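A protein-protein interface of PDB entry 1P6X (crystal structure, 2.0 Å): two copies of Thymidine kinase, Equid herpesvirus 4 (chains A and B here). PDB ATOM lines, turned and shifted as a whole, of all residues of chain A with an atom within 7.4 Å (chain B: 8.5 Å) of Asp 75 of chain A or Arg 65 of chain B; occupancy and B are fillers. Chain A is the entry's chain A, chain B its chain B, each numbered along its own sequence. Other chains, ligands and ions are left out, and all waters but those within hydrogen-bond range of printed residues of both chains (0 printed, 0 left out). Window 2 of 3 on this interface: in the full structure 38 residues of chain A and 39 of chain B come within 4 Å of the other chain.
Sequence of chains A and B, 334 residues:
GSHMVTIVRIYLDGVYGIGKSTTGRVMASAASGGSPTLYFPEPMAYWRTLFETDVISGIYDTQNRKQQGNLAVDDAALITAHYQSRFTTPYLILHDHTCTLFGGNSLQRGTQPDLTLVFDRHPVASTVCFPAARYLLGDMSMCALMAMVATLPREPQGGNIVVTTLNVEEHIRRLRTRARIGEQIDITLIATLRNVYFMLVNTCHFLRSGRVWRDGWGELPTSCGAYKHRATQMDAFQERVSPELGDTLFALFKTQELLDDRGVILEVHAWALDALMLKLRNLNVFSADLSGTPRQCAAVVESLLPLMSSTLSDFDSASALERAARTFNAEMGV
The guanidinium group of Arg 65 of chain B lies within salt-bridge range of the side-chain carboxylate of Asp 75 of chain A (2.6 Å).
The side-chain amide oxygen (OD1) of Asn 70 of chain B sits at hydrogen-bond distance from the guanidinium group (NH2) of Arg 65 of chain B.
N of Leu 71 of chain B is in hydrogen-bond range of O of Arg 65 of chain B (3.3 Å).
Asp 75 of chain B touches Leu 71 of chain A.
CD1 of Leu 71 of chain B touches OD1 of Asp 75 of chain A, at 3.4 Å.
O of Leu 78 of chain A touches CG of His 82 of chain B, 3.6 Å away.
Leu 78 of chain A touches Tyr 83 of chain B.
Leu 78 of chain B touches Ile 79 of chain A (CD1 to CG2, 3.99 Å).
Ile 79 of chain A touches Ile 79 of chain B (CG1 to CG1, 3.7 Å).
CB of Ala 81 of chain A touches NE2 of His 82 of chain B (3.2 Å).
Arg 65 of chain B touches just one residue of chain A: Asp 75.
Of the printed residues of chain A, Leu 78 of chain B touches Ile 79.
Printed residues of chain B within 4 Å of Ala 81 of chain A: His 82.
Printed residues of chain A within 4 Å of Tyr 83 of chain B: Leu 78 (3.9 Å).
Printed residues of chain B within 4 Å of Leu 78 of chain A: His 82 and Tyr 83.
The nearest printed residue of chain B that does not touch Leu 71 of chain A is Leu 71 of chain B (5.5 Å).
Of the 23 printed residues of chain B, 7 touch a printed residue of chain A.
Hydrophobic or aromatic side chains of chain A within 4 Å of the printed part of chain B: Leu 71, Leu 78, Ile 79 and Ala 81.
Leu 71 of chain A touches Asp 75 of chain B, and with the chains exchanged Asp 75 of chain A touches Leu 71 of chain B.
Ile 79 of chain A touches Leu 78 of chain B, but with the chains exchanged Leu 78 of chain A does not touch Ile 79 of chain B (4.1 Å).
Ile 79 of chain B touches its own counterpart, Ile 79 of chain A.
Of the 8 pairs that touch across the chains among the printed residues, 3 have their exchanged pair printed and touching as well.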
ATOM      1  N   THR A  62     -21.795   2.159  34.969  1.00  0.00           N
ATOM      2  CA  THR A  62     -21.366   0.843  34.507  1.00  0.00           C
ATOM      3  C   THR A  62     -20.107   0.402  35.243  1.00  0.00           C
ATOM      4  O   THR A  62     -20.029  -0.742  35.708  1.00  0.00           O
ATOM      5  CB  THR A  62     -21.150   0.852  32.969  1.00  0.00           C
ATOM      6  OG1 THR A  62     -22.396   1.144  32.318  1.00  0.00           O
ATOM      7  CG2 THR A  62     -20.803  -0.528  32.450  1.00  0.00           C
ATOM      8  N   LYS A  66     -19.442  -2.723  38.042  1.00  0.00           N
ATOM      9  CA  LYS A  66     -18.380  -3.682  37.751  1.00  0.00           C
ATOM     10  C   LYS A  66     -17.469  -3.884  38.967  1.00  0.00           C
ATOM     11  O   LYS A  66     -17.231  -5.021  39.380  1.00  0.00           O
ATOM     12  CB  LYS A  66     -17.584  -3.220  36.523  1.00  0.00           C
ATOM     13  CG  LYS A  66     -16.170  -3.769  36.390  1.00  0.00           C
ATOM     14  CD  LYS A  66     -15.472  -3.148  35.191  1.00  0.00           C
ATOM     15  CE  LYS A  66     -14.340  -2.215  35.605  1.00  0.00           C
ATOM     16  NZ  LYS A  66     -13.463  -1.840  34.450  1.00  0.00           N
ATOM     17  N   ASN A  70     -21.940  -6.512  40.721  1.00  0.00           N
ATOM     18  CA  ASN A  70     -23.306  -6.811  40.272  1.00  0.00           C
ATOM     19  C   ASN A  70     -23.342  -6.974  38.742  1.00  0.00           C
ATOM     20  O   ASN A  70     -24.374  -7.321  38.149  1.00  0.00           O
ATOM     21  CB  ASN A  70     -24.325  -5.786  40.842  1.00  0.00           C
ATOM     22  CG  ASN A  70     -25.108  -5.024  39.764  1.00  0.00           C
ATOM     23  OD1 ASN A  70     -24.867  -3.837  39.532  1.00  0.00           O
ATOM     24  ND2 ASN A  70     -26.071  -5.696  39.133  1.00  0.00           N
ATOM     25  N   LEU A  71     -22.178  -6.765  38.132  1.00  0.00           N
ATOM     26  CA  LEU A  71     -22.005  -6.859  36.686  1.00  0.00           C
ATOM     27  C   LEU A  71     -20.618  -7.398  36.360  1.00  0.00           C
ATOM     28  O   LEU A  71     -19.612  -6.861  36.827  1.00  0.00           O
ATOM     29  CB  LEU A  71     -22.210  -5.483  36.037  1.00  0.00           C
ATOM     30  CG  LEU A  71     -22.277  -5.408  34.511  1.00  0.00           C
ATOM     31  CD1 LEU A  71     -23.631  -5.907  34.024  1.00  0.00           C
ATOM     32  CD2 LEU A  71     -22.021  -3.980  34.060  1.00  0.00           C
ATOM     33  N   ALA A  72     -20.574  -8.460  35.560  1.00  0.00           N
ATOM     34  CA  ALA A  72     -19.318  -9.102  35.185  1.00  0.00           C
ATOM     35  C   ALA A  72     -18.423  -8.180  34.348  1.00  0.00           C
ATOM     36  O   ALA A  72     -18.919  -7.309  33.621  1.00  0.00           O
ATOM     37  CB  ALA A  72     -19.596 -10.399  34.432  1.00  0.00           C
ATOM     38  N   VAL A  73     -17.111  -8.381  34.464  1.00  0.00           N
ATOM     39  CA  VAL A  73     -16.114  -7.602  33.718  1.00  0.00           C
ATOM     40  C   VAL A  73     -16.332  -7.675  32.194  1.00  0.00           C
ATOM     41  O   VAL A  73     -16.296  -6.647  31.513  1.00  0.00           O
ATOM     42  CB  VAL A  73     -14.653  -8.007  34.109  1.00  0.00           C
ATOM     43  CG1 VAL A  73     -13.610  -7.204  33.322  1.00  0.00           C
ATOM     44  CG2 VAL A  73     -14.427  -7.822  35.606  1.00  0.00           C
ATOM     45  N   ASP A  74     -16.570  -8.879  31.673  1.00  0.00           N
ATOM     46  CA  ASP A  74     -16.850  -9.081  30.244  1.00  0.00           C
ATOM     47  C   ASP A  74     -18.068  -8.284  29.793  1.00  0.00           C
ATOM     48  O   ASP A  74     -18.030  -7.594  28.774  1.00  0.00           O
ATOM     49  CB  ASP A  74     -17.081 -10.565  29.937  1.00  0.00           C
ATOM     50  CG  ASP A  74     -15.797 -11.369  29.936  1.00  0.00           C
ATOM     51  OD1 ASP A  74     -14.700 -10.756  29.933  1.00  0.00           O
ATOM     52  OD2 ASP A  74     -15.790 -12.625  29.939  1.00  0.00           O
ATOM     53  N   ASP A  75     -19.149  -8.387  30.558  1.00  0.00           N
ATOM     54  CA  ASP A  75     -20.371  -7.671  30.244  1.00  0.00           C
ATOM     55  C   ASP A  75     -20.171  -6.154  30.330  1.00  0.00           C
ATOM     56  O   ASP A  75     -20.667  -5.407  29.470  1.00  0.00           O
ATOM     57  CB  ASP A  75     -21.506  -8.130  31.159  1.00  0.00           C
ATOM     58  CG  ASP A  75     -22.055  -9.500  30.771  1.00  0.00           C
ATOM     59  OD1 ASP A  75     -22.952  -9.988  31.493  1.00  0.00           O
ATOM     60  OD2 ASP A  75     -21.667 -10.162  29.776  1.00  0.00           O
ATOM     61  N   ALA A  76     -19.437  -5.710  31.353  1.00  0.00           N
ATOM     62  CA  ALA A  76     -19.191  -4.284  31.576  1.00  0.00           C
ATOM     63  C   ALA A  76     -18.432  -3.670  30.405  1.00  0.00           C
ATOM     64  O   ALA A  76     -18.794  -2.600  29.918  1.00  0.00           O
ATOM     65  CB  ALA A  76     -18.429  -4.060  32.886  1.00  0.00           C
ATOM     66  N   ALA A  77     -17.397  -4.366  29.947  1.00  0.00           N
ATOM     67  CA  ALA A  77     -16.594  -3.911  28.814  1.00  0.00           C
ATOM     68  C   ALA A  77     -17.497  -3.652  27.596  1.00  0.00           C
ATOM     69  O   ALA A  77     -17.403  -2.598  26.940  1.00  0.00           O
ATOM     70  CB  ALA A  77     -15.515  -4.926  28.496  1.00  0.00           C
ATOM     71  N   LEU A  78     -18.408  -4.591  27.340  1.00  0.00           N
ATOM     72  CA  LEU A  78     -19.390  -4.459  26.261  1.00  0.00           C
ATOM     73  C   LEU A  78     -20.380  -3.322  26.455  1.00  0.00           C
ATOM     74  O   LEU A  78     -20.679  -2.607  25.511  1.00  0.00           O
ATOM     75  CB  LEU A  78     -20.159  -5.776  26.051  1.00  0.00           C
ATOM     76  CG  LEU A  78     -19.318  -7.033  25.872  1.00  0.00           C
ATOM     77  CD1 LEU A  78     -20.201  -8.264  25.995  1.00  0.00           C
ATOM     78  CD2 LEU A  78     -18.553  -7.045  24.555  1.00  0.00           C
ATOM     79  N   ILE A  79     -20.897  -3.155  27.668  1.00  0.00           N
ATOM     80  CA  ILE A  79     -21.861  -2.087  27.937  1.00  0.00           C
ATOM     81  C   ILE A  79     -21.183  -0.705  27.841  1.00  0.00           C
ATOM     82  O   ILE A  79     -21.783   0.256  27.361  1.00  0.00           O
ATOM     83  CB  ILE A  79     -22.553  -2.304  29.311  1.00  0.00           C
ATOM     84  CG1 ILE A  79     -23.484  -3.515  29.243  1.00  0.00           C
ATOM     85  CG2 ILE A  79     -23.370  -1.096  29.734  1.00  0.00           C
ATOM     86  CD1 ILE A  79     -23.453  -4.368  30.510  1.00  0.00           C
ATOM     87  N   THR A  80     -19.920  -0.637  28.258  1.00  0.00           N
ATOM     88  CA  THR A  80     -19.146   0.604  28.188  1.00  0.00           C
ATOM     89  C   THR A  80     -18.975   1.035  26.745  1.00  0.00           C
ATOM     90  O   THR A  80     -19.151   2.205  26.408  1.00  0.00           O
ATOM     91  CB  THR A  80     -17.765   0.412  28.834  1.00  0.00           C
ATOM     92  OG1 THR A  80     -17.946   0.215  30.243  1.00  0.00           O
ATOM     93  CG2 THR A  80     -16.917   1.709  28.730  1.00  0.00           C
ATOM     94  N   ALA A  81     -18.656   0.066  25.897  1.00  0.00           N
ATOM     95  CA  ALA A  81     -18.460   0.353  24.499  1.00  0.00           C
ATOM     96  C   ALA A  81     -19.766   0.878  23.908  1.00  0.00           C
ATOM     97  O   ALA A  81     -19.761   1.843  23.150  1.00  0.00           O
ATOM     98  CB  ALA A  81     -17.962  -0.871  23.773  1.00  0.00           C
ATOM     99  N   SER B  57     -22.084 -15.722  17.501  1.00  0.00           N
ATOM    100  CA  SER B  57     -22.565 -16.467  18.672  1.00  0.00           C
ATOM    101  C   SER B  57     -22.941 -15.529  19.833  1.00  0.00           C
ATOM    102  O   SER B  57     -23.899 -15.786  20.565  1.00  0.00           O
ATOM    103  CB  SER B  57     -21.578 -17.545  19.101  1.00  0.00           C
ATOM    104  OG  SER B  57     -20.286 -17.012  19.304  1.00  0.00           O
ATOM    105  N   GLY B  58     -22.215 -14.421  19.962  1.00  0.00           N
ATOM    106  CA  GLY B  58     -22.421 -13.481  21.054  1.00  0.00           C
ATOM    107  C   GLY B  58     -23.765 -12.799  21.005  1.00  0.00           C
ATOM    108  O   GLY B  58     -24.411 -12.617  22.043  1.00  0.00           O
ATOM    109  N   ILE B  59     -24.208 -12.424  19.809  1.00  0.00           N
ATOM    110  CA  ILE B  59     -25.508 -11.778  19.695  1.00  0.00           C
ATOM    111  C   ILE B  59     -26.639 -12.787  19.982  1.00  0.00           C
ATOM    112  O   ILE B  59     -27.614 -12.459  20.674  1.00  0.00           O
ATOM    113  CB  ILE B  59     -25.651 -10.958  18.350  1.00  0.00           C
ATOM    114  CG1 ILE B  59     -26.678  -9.834  18.501  1.00  0.00           C
ATOM    115  CG2 ILE B  59     -25.923 -11.857  17.122  1.00  0.00           C
ATOM    116  CD1 ILE B  59     -26.642  -8.748  17.383  1.00  0.00           C
ATOM    117  N   TYR B  60     -26.469 -14.020  19.507  1.00  0.00           N
ATOM    118  CA  TYR B  60     -27.412 -15.117  19.828  1.00  0.00           C
ATOM    119  C   TYR B  60     -27.418 -15.462  21.334  1.00  0.00           C
ATOM    120  O   TYR B  60     -28.452 -15.327  21.977  1.00  0.00           O
ATOM    121  CB  TYR B  60     -27.137 -16.364  18.975  1.00  0.00           C
ATOM    122  CG  TYR B  60     -28.167 -17.476  19.114  1.00  0.00           C
ATOM    123  CD1 TYR B  60     -29.501 -17.199  19.449  1.00  0.00           C
ATOM    124  CD2 TYR B  60     -27.803 -18.810  18.912  1.00  0.00           C
ATOM    125  CE1 TYR B  60     -30.447 -18.220  19.587  1.00  0.00           C
ATOM    126  CE2 TYR B  60     -28.741 -19.844  19.039  1.00  0.00           C
ATOM    127  CZ  TYR B  60     -30.063 -19.540  19.376  1.00  0.00           C
ATOM    128  OH  TYR B  60     -31.004 -20.558  19.502  1.00  0.00           O
ATOM    129  N   ASP B  61     -26.267 -15.882  21.875  1.00  0.00           N
ATOM    130  CA  ASP B  61     -26.055 -16.076  23.330  1.00  0.00           C
ATOM    131  C   ASP B  61     -26.689 -14.984  24.220  1.00  0.00           C
ATOM    132  O   ASP B  61     -27.233 -15.290  25.292  1.00  0.00           O
ATOM    133  CB  ASP B  61     -24.550 -16.154  23.630  1.00  0.00           C
ATOM    134  CG  ASP B  61     -24.008 -17.576  23.605  1.00  0.00           C
ATOM    135  OD1 ASP B  61     -24.238 -18.308  22.609  1.00  0.00           O
ATOM    136  OD2 ASP B  61     -23.326 -18.048  24.544  1.00  0.00           O
ATOM    137  N   THR B  62     -26.622 -13.723  23.785  1.00  0.00           N
ATOM    138  CA  THR B  62     -27.222 -12.617  24.543  1.00  0.00           C
ATOM    139  C   THR B  62     -28.731 -12.759  24.682  1.00  0.00           C
ATOM    140  O   THR B  62     -29.286 -12.537  25.762  1.00  0.00           O
ATOM    141  CB  THR B  62     -26.893 -11.254  23.900  1.00  0.00           C
ATOM    142  OG1 THR B  62     -25.478 -11.048  23.933  1.00  0.00           O
ATOM    143  CG2 THR B  62     -27.443 -10.107  24.761  1.00  0.00           C
ATOM    144  N   GLN B  63     -29.392 -13.097  23.577  1.00  0.00           N
ATOM    145  CA  GLN B  63     -30.837 -13.323  23.585  1.00  0.00           C
ATOM    146  C   GLN B  63     -31.189 -14.538  24.455  1.00  0.00           C
ATOM    147  O   GLN B  63     -32.244 -14.568  25.084  1.00  0.00           O
ATOM    148  CB  GLN B  63     -31.381 -13.513  22.165  1.00  0.00           C
ATOM    149  CG  GLN B  63     -30.850 -12.556  21.102  1.00  0.00           C
ATOM    150  CD  GLN B  63     -30.690 -11.116  21.585  1.00  0.00           C
ATOM    151  OE1 GLN B  63     -31.626 -10.517  22.136  1.00  0.00           O
ATOM    152  NE2 GLN B  63     -29.497 -10.560  21.382  1.00  0.00           N
ATOM    153  N   ASN B  64     -30.298 -15.525  24.479  1.00  0.00           N
ATOM    154  CA  ASN B  64     -30.486 -16.733  25.285  1.00  0.00           C
ATOM    155  C   ASN B  64     -30.403 -16.467  26.789  1.00  0.00           C
ATOM    156  O   ASN B  64     -31.221 -16.979  27.556  1.00  0.00           O
ATOM    157  CB  ASN B  64     -29.497 -17.824  24.868  1.00  0.00           C
ATOM    158  CG  ASN B  64     -29.952 -18.577  23.627  1.00  0.00           C
ATOM    159  OD1 ASN B  64     -30.982 -18.249  23.027  1.00  0.00           O
ATOM    160  ND2 ASN B  64     -29.178 -19.586  23.229  1.00  0.00           N
ATOM    161  N   ARG B  65     -29.420 -15.661  27.191  1.00  0.00           N
ATOM    162  CA  ARG B  65     -29.263 -15.235  28.578  1.00  0.00           C
ATOM    163  C   ARG B  65     -30.427 -14.358  29.039  1.00  0.00           C
ATOM    164  O   ARG B  65     -30.847 -14.431  30.198  1.00  0.00           O
ATOM    165  CB  ARG B  65     -27.953 -14.468  28.762  1.00  0.00           C
ATOM    166  CG  ARG B  65     -26.695 -15.280  28.553  1.00  0.00           C
ATOM    167  CD  ARG B  65     -25.443 -14.434  28.448  1.00  0.00           C
ATOM    168  NE  ARG B  65     -25.146 -13.764  29.709  1.00  0.00           N
ATOM    169  CZ  ARG B  65     -24.275 -12.770  29.864  1.00  0.00           C
ATOM    170  NH1 ARG B  65     -23.593 -12.293  28.828  1.00  0.00           N
ATOM    171  NH2 ARG B  65     -24.085 -12.249  31.068  1.00  0.00           N
ATOM    172  N   LYS B  66     -30.917 -13.508  28.134  1.00  0.00           N
ATOM    173  CA  LYS B  66     -32.082 -12.668  28.388  1.00  0.00           C
ATOM    174  C   LYS B  66     -33.300 -13.568  28.629  1.00  0.00           C
ATOM    175  O   LYS B  66     -33.982 -13.448  29.659  1.00  0.00           O
ATOM    176  CB  LYS B  66     -32.313 -11.721  27.202  1.00  0.00           C
ATOM    177  CG  LYS B  66     -33.639 -10.955  27.205  1.00  0.00           C
ATOM    178  CD  LYS B  66     -33.793 -10.055  25.961  1.00  0.00           C
ATOM    179  CE  LYS B  66     -34.080 -10.855  24.678  1.00  0.00           C
ATOM    180  NZ  LYS B  66     -35.063 -10.200  23.758  1.00  0.00           N
ATOM    181  N   GLN B  67     -33.526 -14.493  27.690  1.00  0.00           N
ATOM    182  CA  GLN B  67     -34.679 -15.398  27.701  1.00  0.00           C
ATOM    183  C   GLN B  67     -34.569 -16.488  28.781  1.00  0.00           C
ATOM    184  O   GLN B  67     -35.210 -17.544  28.686  1.00  0.00           O
ATOM    185  CB  GLN B  67     -34.869 -16.035  26.313  1.00  0.00           C
ATOM    186  CG  GLN B  67     -35.639 -15.163  25.300  1.00  0.00           C
ATOM    187  CD  GLN B  67     -35.712 -15.780  23.897  1.00  0.00           C
ATOM    188  OE1 GLN B  67     -35.206 -16.884  23.663  1.00  0.00           O
ATOM    189  NE2 GLN B  67     -36.337 -15.063  22.964  1.00  0.00           N
ATOM    190  N   GLN B  68     -33.765 -16.206  29.807  1.00  0.00           N
ATOM    191  CA  GLN B  68     -33.483 -17.135  30.891  1.00  0.00           C
ATOM    192  C   GLN B  68     -33.087 -16.369  32.159  1.00  0.00           C
ATOM    193  O   GLN B  68     -33.488 -15.216  32.362  1.00  0.00           O
ATOM    194  CB  GLN B  68     -32.338 -18.066  30.491  1.00  0.00           C
ATOM    195  CG  GLN B  68     -32.746 -19.260  29.660  1.00  0.00           C
ATOM    196  CD  GLN B  68     -31.730 -20.374  29.724  1.00  0.00           C
ATOM    197  OE1 GLN B  68     -30.535 -20.128  29.947  1.00  0.00           O
ATOM    198  NE2 GLN B  68     -32.194 -21.609  29.536  1.00  0.00           N
ATOM    199  N   GLY B  69     -32.292 -17.023  33.004  1.00  0.00           N
ATOM    200  CA  GLY B  69     -31.730 -16.395  34.186  1.00  0.00           C
ATOM    201  C   GLY B  69     -30.714 -15.302  33.875  1.00  0.00           C
ATOM    202  O   GLY B  69     -31.040 -14.119  33.930  1.00  0.00           O
ATOM    203  N   ASN B  70     -29.501 -15.730  33.528  1.00  0.00           N
ATOM    204  CA  ASN B  70     -28.283 -14.904  33.427  1.00  0.00           C
ATOM    205  C   ASN B  70     -28.361 -13.360  33.363  1.00  0.00           C
ATOM    206  O   ASN B  70     -27.655 -12.684  34.125  1.00  0.00           O
ATOM    207  CB  ASN B  70     -27.387 -15.432  32.286  1.00  0.00           C
ATOM    208  CG  ASN B  70     -25.889 -15.426  32.640  1.00  0.00           C
ATOM    209  OD1 ASN B  70     -25.386 -14.514  33.314  1.00  0.00           O
ATOM    210  ND2 ASN B  70     -25.169 -16.445  32.164  1.00  0.00           N
ATOM    211  N   LEU B  71     -29.182 -12.802  32.470  1.00  0.00           N
ATOM    212  CA  LEU B  71     -29.027 -11.387  32.089  1.00  0.00           C
ATOM    213  C   LEU B  71     -30.323 -10.569  32.009  1.00  0.00           C
ATOM    214  O   LEU B  71     -31.304 -11.007  31.407  1.00  0.00           O
ATOM    215  CB  LEU B  71     -28.263 -11.305  30.755  1.00  0.00           C
ATOM    216  CG  LEU B  71     -27.610  -9.998  30.296  1.00  0.00           C
ATOM    217  CD1 LEU B  71     -26.350  -9.698  31.090  1.00  0.00           C
ATOM    218  CD2 LEU B  71     -27.285 -10.106  28.820  1.00  0.00           C
ATOM    219  N   ALA B  72     -30.305  -9.379  32.607  1.00  0.00           N
ATOM    220  CA  ALA B  72     -31.473  -8.492  32.629  1.00  0.00           C
ATOM    221  C   ALA B  72     -31.778  -7.874  31.262  1.00  0.00           C
ATOM    222  O   ALA B  72     -30.855  -7.562  30.497  1.00  0.00           O
ATOM    223  CB  ALA B  72     -31.290  -7.403  33.667  1.00  0.00           C
ATOM    224  N   VAL B  73     -33.066  -7.677  30.971  1.00  0.00           N
ATOM    225  CA  VAL B  73     -33.490  -7.203  29.652  1.00  0.00           C
ATOM    226  C   VAL B  73     -32.908  -5.831  29.259  1.00  0.00           C
ATOM    227  O   VAL B  73     -32.620  -5.617  28.086  1.00  0.00           O
ATOM    228  CB  VAL B  73     -35.048  -7.298  29.381  1.00  0.00           C
ATOM    229  CG1 VAL B  73     -35.749  -8.216  30.375  1.00  0.00           C
ATOM    230  CG2 VAL B  73     -35.718  -5.916  29.320  1.00  0.00           C
ATOM    231  N   ASP B  75     -29.877  -4.608  30.243  1.00  0.00           N
ATOM    232  CA  ASP B  75     -28.487  -4.928  29.913  1.00  0.00           C
ATOM    233  C   ASP B  75     -28.344  -5.653  28.558  1.00  0.00           C
ATOM    234  O   ASP B  75     -27.429  -5.348  27.787  1.00  0.00           O
ATOM    235  CB  ASP B  75     -27.838  -5.779  31.016  1.00  0.00           C
ATOM    236  CG  ASP B  75     -27.518  -4.983  32.302  1.00  0.00           C
ATOM    237  OD1 ASP B  75     -27.189  -3.772  32.241  1.00  0.00           O
ATOM    238  OD2 ASP B  75     -27.556  -5.519  33.437  1.00  0.00           O
ATOM    239  N   ALA B  76     -29.243  -6.604  28.280  1.00  0.00           N
ATOM    240  CA  ALA B  76     -29.203  -7.388  27.033  1.00  0.00           C
ATOM    241  C   ALA B  76     -29.402  -6.510  25.812  1.00  0.00           C
ATOM    242  O   ALA B  76     -28.791  -6.746  24.785  1.00  0.00           O
ATOM    243  CB  ALA B  76     -30.258  -8.494  27.037  1.00  0.00           C
ATOM    244  N   LEU B  78     -28.551  -3.306  25.552  1.00  0.00           N
ATOM    245  CA  LEU B  78     -27.305  -2.547  25.344  1.00  0.00           C
ATOM    246  C   LEU B  78     -26.204  -3.412  24.761  1.00  0.00           C
ATOM    247  O   LEU B  78     -25.483  -2.978  23.864  1.00  0.00           O
ATOM    248  CB  LEU B  78     -26.808  -1.892  26.651  1.00  0.00           C
ATOM    249  CG  LEU B  78     -27.801  -1.072  27.477  1.00  0.00           C
ATOM    250  CD1 LEU B  78     -27.265  -0.835  28.903  1.00  0.00           C
ATOM    251  CD2 LEU B  78     -28.164   0.254  26.785  1.00  0.00           C
ATOM    252  N   ILE B  79     -26.076  -4.633  25.277  1.00  0.00           N
ATOM    253  CA  ILE B  79     -25.078  -5.583  24.803  1.00  0.00           C
ATOM    254  C   ILE B  79     -25.370  -6.060  23.360  1.00  0.00           C
ATOM    255  O   ILE B  79     -24.449  -6.283  22.573  1.00  0.00           O
ATOM    256  CB  ILE B  79     -24.965  -6.788  25.787  1.00  0.00           C
ATOM    257  CG1 ILE B  79     -24.241  -6.366  27.073  1.00  0.00           C
ATOM    258  CG2 ILE B  79     -24.229  -7.960  25.159  1.00  0.00           C
ATOM    259  CD1 ILE B  79     -24.658  -7.141  28.310  1.00  0.00           C
ATOM    260  N   HIS B  82     -24.307  -3.369  21.154  1.00  0.00           N
ATOM    261  CA  HIS B  82     -22.867  -3.403  20.975  1.00  0.00           C
ATOM    262  C   HIS B  82     -22.413  -4.459  19.973  1.00  0.00           C
ATOM    263  O   HIS B  82     -21.561  -4.184  19.118  1.00  0.00           O
ATOM    264  CB  HIS B  82     -22.083  -3.563  22.265  1.00  0.00           C
ATOM    265  CG  HIS B  82     -20.611  -3.465  22.034  1.00  0.00           C
ATOM    266  ND1 HIS B  82     -19.759  -4.526  22.225  1.00  0.00           N
ATOM    267  CD2 HIS B  82     -19.864  -2.477  21.487  1.00  0.00           C
ATOM    268  CE1 HIS B  82     -18.535  -4.173  21.880  1.00  0.00           C
ATOM    269  NE2 HIS B  82     -18.572  -2.940  21.414  1.00  0.00           N
ATOM    270  N   TYR B  83     -22.954  -5.677  20.072  1.00  0.00           N
ATOM    271  CA  TYR B  83     -22.608  -6.710  19.087  1.00  0.00           C
ATOM    272  C   TYR B  83     -22.978  -6.296  17.654  1.00  0.00           C
ATOM    273  O   TYR B  83     -22.215  -6.544  16.701  1.00  0.00           O
ATOM    274  CB  TYR B  83     -23.266  -8.047  19.447  1.00  0.00           C
ATOM    275  CG  TYR B  83     -22.453  -8.838  20.451  1.00  0.00           C
ATOM    276  CD1 TYR B  83     -22.983  -9.179  21.705  1.00  0.00           C
ATOM    277  CD2 TYR B  83     -21.155  -9.223  20.167  1.00  0.00           C
ATOM    278  CE1 TYR B  83     -22.233  -9.909  22.637  1.00  0.00           C
ATOM    279  CE2 TYR B  83     -20.397  -9.942  21.087  1.00  0.00           C
ATOM    280  CZ  TYR B  83     -20.952 -10.285  22.321  1.00  0.00           C
ATOM    281  OH  TYR B  83     -20.190 -10.991  23.229  1.00  0.00           O
